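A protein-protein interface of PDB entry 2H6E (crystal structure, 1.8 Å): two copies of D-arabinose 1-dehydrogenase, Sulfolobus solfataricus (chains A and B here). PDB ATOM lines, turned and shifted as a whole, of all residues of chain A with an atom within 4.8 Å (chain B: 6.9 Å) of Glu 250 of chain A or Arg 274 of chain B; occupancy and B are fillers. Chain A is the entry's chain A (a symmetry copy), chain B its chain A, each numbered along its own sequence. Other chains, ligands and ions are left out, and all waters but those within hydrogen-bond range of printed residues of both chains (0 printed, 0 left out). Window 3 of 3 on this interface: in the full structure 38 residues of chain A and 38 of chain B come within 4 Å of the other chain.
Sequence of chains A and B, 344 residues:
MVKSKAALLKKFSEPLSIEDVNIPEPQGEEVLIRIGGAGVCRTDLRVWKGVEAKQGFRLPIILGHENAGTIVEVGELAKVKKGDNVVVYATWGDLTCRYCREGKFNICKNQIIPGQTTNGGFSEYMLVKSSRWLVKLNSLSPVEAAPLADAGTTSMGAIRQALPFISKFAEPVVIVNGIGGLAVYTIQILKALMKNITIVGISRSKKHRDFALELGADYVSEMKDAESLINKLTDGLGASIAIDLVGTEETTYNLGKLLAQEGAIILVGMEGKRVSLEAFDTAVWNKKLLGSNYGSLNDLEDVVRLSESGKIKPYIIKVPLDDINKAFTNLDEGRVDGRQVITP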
ATOM      1  N   THR A 248     -14.080 -24.510 -31.388  1.00  0.00           N
ATOM      2  CA  THR A 248     -12.814 -25.025 -31.890  1.00  0.00           C
ATOM      3  C   THR A 248     -11.685 -24.105 -31.466  1.00  0.00           C
ATOM      4  O   THR A 248     -11.917 -23.007 -30.913  1.00  0.00           O
ATOM      5  CB  THR A 248     -12.811 -25.152 -33.444  1.00  0.00           C
ATOM      6  OG1 THR A 248     -12.913 -23.844 -34.037  1.00  0.00           O
ATOM      7  CG2 THR A 248     -13.962 -26.026 -33.921  1.00  0.00           C
ATOM      8  N   GLU A 249     -10.465 -24.560 -31.750  1.00  0.00           N
ATOM      9  CA  GLU A 249      -9.247 -23.816 -31.495  1.00  0.00           C
ATOM     10  C   GLU A 249      -9.374 -22.397 -32.100  1.00  0.00           C
ATOM     11  O   GLU A 249      -9.027 -21.374 -31.467  1.00  0.00           O
ATOM     12  CB  GLU A 249      -8.051 -24.598 -32.087  1.00  0.00           C
ATOM     13  CG  GLU A 249      -7.769 -26.038 -31.473  1.00  0.00           C
ATOM     14  CD  GLU A 249      -8.611 -27.209 -32.055  1.00  0.00           C
ATOM     15  OE1 GLU A 249      -9.516 -26.959 -32.888  1.00  0.00           O
ATOM     16  OE2 GLU A 249      -8.365 -28.393 -31.668  1.00  0.00           O
ATOM     17  N   GLU A 250      -9.884 -22.334 -33.327  1.00  0.00           N
ATOM     18  CA  GLU A 250      -9.979 -21.046 -34.024  1.00  0.00           C
ATOM     19  C   GLU A 250     -11.156 -20.163 -33.584  1.00  0.00           C
ATOM     20  O   GLU A 250     -11.002 -18.941 -33.521  1.00  0.00           O
ATOM     21  CB  GLU A 250      -9.980 -21.237 -35.543  1.00  0.00           C
ATOM     22  CG  GLU A 250      -8.567 -21.374 -36.140  1.00  0.00           C
ATOM     23  CD  GLU A 250      -7.580 -20.336 -35.579  1.00  0.00           C
ATOM     24  OE1 GLU A 250      -7.535 -19.190 -36.092  1.00  0.00           O
ATOM     25  OE2 GLU A 250      -6.855 -20.676 -34.613  1.00  0.00           O
ATOM     26  N   THR A 251     -12.308 -20.757 -33.272  1.00  0.00           N
ATOM     27  CA  THR A 251     -13.471 -19.956 -32.870  1.00  0.00           C
ATOM     28  C   THR A 251     -13.211 -19.208 -31.567  1.00  0.00           C
ATOM     29  O   THR A 251     -13.432 -18.010 -31.496  1.00  0.00           O
ATOM     30  CB  THR A 251     -14.785 -20.780 -32.759  1.00  0.00           C
ATOM     31  OG1 THR A 251     -14.679 -21.724 -31.693  1.00  0.00           O
ATOM     32  CG2 THR A 251     -15.092 -21.505 -34.065  1.00  0.00           C
ATOM     33  N   THR A 252     -12.715 -19.888 -30.544  1.00  0.00           N
ATOM     34  CA  THR A 252     -12.489 -19.214 -29.262  1.00  0.00           C
ATOM     35  C   THR A 252     -11.382 -18.157 -29.368  1.00  0.00           C
ATOM     36  O   THR A 252     -11.522 -17.034 -28.886  1.00  0.00           O
ATOM     37  CB  THR A 252     -12.179 -20.207 -28.138  1.00  0.00           C
ATOM     38  OG1 THR A 252     -11.054 -21.017 -28.482  1.00  0.00           O
ATOM     39  CG2 THR A 252     -13.427 -21.096 -27.839  1.00  0.00           C
ATOM     40  N   TYR A 253     -10.286 -18.511 -30.032  1.00  0.00           N
ATOM     41  CA  TYR A 253      -9.206 -17.558 -30.258  1.00  0.00           C
ATOM     42  C   TYR A 253      -9.735 -16.246 -30.856  1.00  0.00           C
ATOM     43  O   TYR A 253      -9.448 -15.153 -30.351  1.00  0.00           O
ATOM     44  CB  TYR A 253      -8.148 -18.175 -31.157  1.00  0.00           C
ATOM     45  CG  TYR A 253      -6.976 -17.258 -31.396  1.00  0.00           C
ATOM     46  CD1 TYR A 253      -5.904 -17.233 -30.513  1.00  0.00           C
ATOM     47  CD2 TYR A 253      -6.950 -16.405 -32.492  1.00  0.00           C
ATOM     48  CE1 TYR A 253      -4.816 -16.380 -30.723  1.00  0.00           C
ATOM     49  CE2 TYR A 253      -5.866 -15.536 -32.706  1.00  0.00           C
ATOM     50  CZ  TYR A 253      -4.808 -15.535 -31.817  1.00  0.00           C
ATOM     51  OH  TYR A 253      -3.730 -14.698 -32.020  1.00  0.00           O
ATOM     52  N   ASN A 254     -10.526 -16.357 -31.919  1.00  0.00           N
ATOM     53  CA  ASN A 254     -11.031 -15.186 -32.633  1.00  0.00           C
ATOM     54  C   ASN A 254     -12.089 -14.409 -31.850  1.00  0.00           C
ATOM     55  O   ASN A 254     -12.067 -13.163 -31.824  1.00  0.00           O
ATOM     56  CB  ASN A 254     -11.553 -15.612 -34.012  1.00  0.00           C
ATOM     57  CG  ASN A 254     -10.424 -15.959 -34.978  1.00  0.00           C
ATOM     58  OD1 ASN A 254      -9.382 -15.309 -34.988  1.00  0.00           O
ATOM     59  ND2 ASN A 254     -10.628 -16.987 -35.785  1.00  0.00           N
ATOM     60  N   SER A 276      -8.500 -22.474 -27.756  1.00  0.00           N
ATOM     61  CA  SER A 276      -7.296 -21.706 -27.574  1.00  0.00           C
ATOM     62  C   SER A 276      -7.612 -20.216 -27.484  1.00  0.00           C
ATOM     63  O   SER A 276      -8.656 -19.756 -27.956  1.00  0.00           O
ATOM     64  CB  SER A 276      -6.273 -22.010 -28.672  1.00  0.00           C
ATOM     65  OG  SER A 276      -6.431 -21.179 -29.798  1.00  0.00           O
ATOM     66  N   LEU A 277      -6.735 -19.502 -26.799  1.00  0.00           N
ATOM     67  CA  LEU A 277      -6.864 -18.068 -26.610  1.00  0.00           C
ATOM     68  C   LEU A 277      -5.470 -17.465 -26.638  1.00  0.00           C
ATOM     69  O   LEU A 277      -4.504 -18.071 -26.174  1.00  0.00           O
ATOM     70  CB  LEU A 277      -7.493 -17.737 -25.265  1.00  0.00           C
ATOM     71  CG  LEU A 277      -8.891 -18.271 -24.956  1.00  0.00           C
ATOM     72  CD1 LEU A 277      -9.188 -18.103 -23.463  1.00  0.00           C
ATOM     73  CD2 LEU A 277      -9.934 -17.581 -25.805  1.00  0.00           C
ATOM     74  N   GLU A 278      -5.382 -16.263 -27.168  1.00  0.00           N
ATOM     75  CA  GLU A 278      -4.162 -15.478 -27.068  1.00  0.00           C
ATOM     76  C   GLU A 278      -3.892 -15.143 -25.602  1.00  0.00           C
ATOM     77  O   GLU A 278      -4.760 -14.596 -24.900  1.00  0.00           O
ATOM     78  CB  GLU A 278      -4.288 -14.186 -27.869  1.00  0.00           C
ATOM     79  CG  GLU A 278      -2.928 -13.517 -28.068  1.00  0.00           C
ATOM     80  CD  GLU A 278      -3.022 -12.115 -28.563  1.00  0.00           C
ATOM     81  OE1 GLU A 278      -3.018 -11.918 -29.798  1.00  0.00           O
ATOM     82  OE2 GLU A 278      -3.095 -11.198 -27.719  1.00  0.00           O
ATOM     83  N   ALA A 279      -2.695 -15.480 -25.142  1.00  0.00           N
ATOM     84  CA  ALA A 279      -2.316 -15.259 -23.751  1.00  0.00           C
ATOM     85  C   ALA A 279      -2.324 -13.779 -23.379  1.00  0.00           C
ATOM     86  O   ALA A 279      -2.870 -13.411 -22.353  1.00  0.00           O
ATOM     87  CB  ALA A 279      -0.966 -15.892 -23.453  1.00  0.00           C
ATOM     88  N   GLY B 247       1.700 -19.710 -17.843  1.00  0.00           N
ATOM     89  CA  GLY B 247       0.771 -19.367 -18.885  1.00  0.00           C
ATOM     90  C   GLY B 247       1.210 -19.730 -20.284  1.00  0.00           C
ATOM     91  O   GLY B 247       1.374 -18.847 -21.129  1.00  0.00           O
ATOM     92  N   THR B 248       1.400 -21.024 -20.530  1.00  0.00           N
ATOM     93  CA  THR B 248       1.657 -21.516 -21.876  1.00  0.00           C
ATOM     94  C   THR B 248       0.532 -22.440 -22.305  1.00  0.00           C
ATOM     95  O   THR B 248      -0.356 -22.796 -21.500  1.00  0.00           O
ATOM     96  CB  THR B 248       3.010 -22.287 -21.967  1.00  0.00           C
ATOM     97  OG1 THR B 248       2.941 -23.481 -21.168  1.00  0.00           O
ATOM     98  CG2 THR B 248       4.165 -21.415 -21.496  1.00  0.00           C
ATOM     99  N   GLU B 249       0.595 -22.833 -23.577  1.00  0.00           N
ATOM    100  CA  GLU B 249      -0.338 -23.766 -24.179  1.00  0.00           C
ATOM    101  C   GLU B 249      -0.438 -25.034 -23.298  1.00  0.00           C
ATOM    102  O   GLU B 249      -1.540 -25.559 -23.016  1.00  0.00           O
ATOM    103  CB  GLU B 249       0.138 -24.089 -25.616  1.00  0.00           C
ATOM    104  CG  GLU B 249       0.191 -22.871 -26.639  1.00  0.00           C
ATOM    105  CD  GLU B 249       1.473 -21.991 -26.588  1.00  0.00           C
ATOM    106  OE1 GLU B 249       2.337 -22.214 -25.707  1.00  0.00           O
ATOM    107  OE2 GLU B 249       1.611 -21.061 -27.442  1.00  0.00           O
ATOM    108  N   GLU B 250       0.716 -25.523 -22.853  1.00  0.00           N
ATOM    109  CA  GLU B 250       0.742 -26.765 -22.071  1.00  0.00           C
ATOM    110  C   GLU B 250       0.340 -26.604 -20.598  1.00  0.00           C
ATOM    111  O   GLU B 250      -0.316 -27.494 -20.051  1.00  0.00           O
ATOM    112  CB  GLU B 250       2.096 -27.469 -22.195  1.00  0.00           C
ATOM    113  CG  GLU B 250       2.212 -28.345 -23.455  1.00  0.00           C
ATOM    114  CD  GLU B 250       0.965 -29.209 -23.699  1.00  0.00           C
ATOM    115  OE1 GLU B 250       0.858 -30.315 -23.110  1.00  0.00           O
ATOM    116  OE2 GLU B 250       0.088 -28.769 -24.480  1.00  0.00           O
ATOM    117  N   THR B 252      -1.832 -24.412 -19.109  1.00  0.00           N
ATOM    118  CA  THR B 252      -3.278 -24.278 -18.910  1.00  0.00           C
ATOM    119  C   THR B 252      -4.017 -25.579 -19.253  1.00  0.00           C
ATOM    120  O   THR B 252      -4.885 -26.035 -18.511  1.00  0.00           O
ATOM    121  CB  THR B 252      -3.861 -23.104 -19.703  1.00  0.00           C
ATOM    122  OG1 THR B 252      -3.558 -23.240 -21.093  1.00  0.00           O
ATOM    123  CG2 THR B 252      -3.316 -21.751 -19.149  1.00  0.00           C
ATOM    124  N   GLU B 271       3.688 -16.443 -20.743  1.00  0.00           N
ATOM    125  CA  GLU B 271       4.975 -16.801 -21.351  1.00  0.00           C
ATOM    126  C   GLU B 271       4.788 -17.400 -22.727  1.00  0.00           C
ATOM    127  O   GLU B 271       5.645 -17.228 -23.576  1.00  0.00           O
ATOM    128  CB  GLU B 271       5.772 -17.749 -20.454  1.00  0.00           C
ATOM    129  CG  GLU B 271       6.250 -17.040 -19.208  1.00  0.00           C
ATOM    130  CD  GLU B 271       7.143 -17.870 -18.321  1.00  0.00           C
ATOM    131  OE1 GLU B 271       7.702 -18.885 -18.790  1.00  0.00           O
ATOM    132  OE2 GLU B 271       7.289 -17.488 -17.141  1.00  0.00           O
ATOM    133  N   GLY B 272       3.672 -18.094 -22.946  1.00  0.00           N
ATOM    134  CA  GLY B 272       3.322 -18.615 -24.265  1.00  0.00           C
ATOM    135  C   GLY B 272       2.561 -17.619 -25.129  1.00  0.00           C
ATOM    136  O   GLY B 272       2.042 -16.614 -24.634  1.00  0.00           O
ATOM    137  N   LYS B 273       2.500 -17.890 -26.432  1.00  0.00           N
ATOM    138  CA  LYS B 273       1.716 -17.052 -27.344  1.00  0.00           C
ATOM    139  C   LYS B 273       0.229 -17.254 -27.083  1.00  0.00           C
ATOM    140  O   LYS B 273      -0.563 -16.301 -27.073  1.00  0.00           O
ATOM    141  CB  LYS B 273       2.036 -17.387 -28.809  1.00  0.00           C
ATOM    142  CG  LYS B 273       1.931 -16.198 -29.764  1.00  0.00           C
ATOM    143  N   ARG B 274      -0.132 -18.515 -26.895  1.00  0.00           N
ATOM    144  CA  ARG B 274      -1.496 -18.901 -26.663  1.00  0.00           C
ATOM    145  C   ARG B 274      -1.588 -19.754 -25.417  1.00  0.00           C
ATOM    146  O   ARG B 274      -0.589 -20.263 -24.913  1.00  0.00           O
ATOM    147  CB  ARG B 274      -2.035 -19.660 -27.873  1.00  0.00           C
ATOM    148  CG  ARG B 274      -2.374 -18.723 -29.036  1.00  0.00           C
ATOM    149  CD  ARG B 274      -2.253 -19.375 -30.377  1.00  0.00           C
ATOM    150  NE  ARG B 274      -3.530 -19.891 -30.862  1.00  0.00           N
ATOM    151  CZ  ARG B 274      -4.141 -19.511 -31.986  1.00  0.00           C
ATOM    152  NH1 ARG B 274      -3.614 -18.589 -32.792  1.00  0.00           N
ATOM    153  NH2 ARG B 274      -5.298 -20.071 -32.319  1.00  0.00           N
ATOM    154  N   VAL B 275      -2.803 -19.847 -24.909  1.00  0.00           N
ATOM    155  CA  VAL B 275      -3.150 -20.844 -23.923  1.00  0.00           C
ATOM    156  C   VAL B 275      -4.152 -21.793 -24.581  1.00  0.00           C
ATOM    157  O   VAL B 275      -4.772 -21.458 -25.597  1.00  0.00           O
ATOM    158  CB  VAL B 275      -3.710 -20.208 -22.657  1.00  0.00           C
ATOM    159  CG1 VAL B 275      -2.580 -19.460 -21.917  1.00  0.00           C
ATOM    160  CG2 VAL B 275      -4.909 -19.261 -22.971  1.00  0.00           C
ATOM    161  N   SER B 276      -4.300 -22.981 -24.017  1.00  0.00           N
ATOM    162  CA  SER B 276      -5.177 -23.965 -24.597  1.00  0.00           C
ATOM    163  C   SER B 276      -5.830 -24.814 -23.509  1.00  0.00           C
ATOM    164  O   SER B 276      -5.320 -24.922 -22.391  1.00  0.00           O
ATOM    165  CB  SER B 276      -4.443 -24.823 -25.631  1.00  0.00           C
ATOM    166  OG  SER B 276      -3.833 -25.954 -25.055  1.00  0.00           O
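O of Lys 273 of chain B sits at hydrogen-bond distance from N of Ala 279 of chain A, 3.0 Å away.
The side-chain carboxylate (OE2) of Glu 250 of chain A is in salt-bridge range of the guanidinium group (NH2) of Arg 274 of chain B (2.8 Å).
The guanidinium group of Arg 274 of chain B lies within hydrogen-bond range of the side-chain hydroxyl of Ser 276 of chain A, at 3.0 Å.
The backbone NH of Val 275 of chain B sits at hydrogen-bond distance from the backbone carbonyl oxygen of Leu 277 of chain A.
The backbone carbonyl oxygen of Gly 247 of chain B sits at hydrogen-bond distance from the backbone NH of Gly 272 of chain B, at 3.0 Å.
The side-chain carboxylate of Glu 249 of chain B is in hydrogen-bond range of the backbone NH of Lys 273 of chain B, 3.4 Å away.
O of Arg 274 of chain B lies within hydrogen-bond range of N of Glu 249 of chain B (3.1 Å).
The side-chain hydroxyl (OG1) of Thr 248 of chain A sits close to the backbone NH (N) of Glu 250 of chain A, at 3.5 Å.
The side-chain hydroxyl (OG) of Ser 276 of chain A sits at hydrogen-bond distance from the backbone carbonyl oxygen (O) of Glu 249 of chain A (3.1 Å).
The backbone carbonyl oxygen of Glu 250 of chain A lies within hydrogen-bond range of the side-chain amide nitrogen of Asn 254 of chain A, 3.0 Å away.
Tyr 253 of chain A touches Arg 274 of chain B (CD1 to CZ, 3.2 Å).
Val 275 of chain B touches Ser 276 of chain A (O to CA, 3.2 Å).
Leu 277 of chain A touches Arg 274 of chain B.
CA of Glu 278 of chain A touches O of Lys 273 of chain B, at 3.7 Å.
CB of Ala 279 of chain A touches O of Gly 272 of chain B, at 3.3 Å.
CA of Arg 274 of chain B touches N of Ala 279 of chain A, 3.9 Å away.
Glu 249 of chain A touches none of the printed residues of chain B.
Of chain B, only Arg 274 (2.8 Å) comes within 4 Å of Glu 250 of chain A.
Of the printed residues of chain B, Leu 277 of chain A touches Arg 274 and Val 275.
Arg 274 of chain B touches just these residues of chain A: Glu 250 (2.8 Å), Tyr 253 (3.2 Å), Ser 276 (3.0 Å), Leu 277 (3.2 Å) and Ala 279 (3.9 Å).
Of the printed residues of chain A, Val 275 of chain B touches Ser 276 (3.2 Å) and Leu 277 (2.8 Å).
The nearest printed residue of chain A that does not touch Arg 274 of chain B is Glu 249 of chain A (4.04 Å).
Hydrophobic or aromatic side chains of chain B within 4 Å of the printed part of chain A: Val 275.
Hydrophobic or aromatic side chains of chain A within 4 Å of the printed part of chain B: Tyr 253, Leu 277 and Ala 279.
Among the printed residues, Asp or Glu carboxylates within 4 Å of a Lys or Arg side-chain nitrogen of the other chain: Glu 250 of chain A with Arg 274 of chain B (2.8 Å).
Positions printed for both chains: 248, 249, 250, 252 and 276.
Of the 10 pairs that touch across the chains among the printed residues, none has its exchanged pair printed and touching as well.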
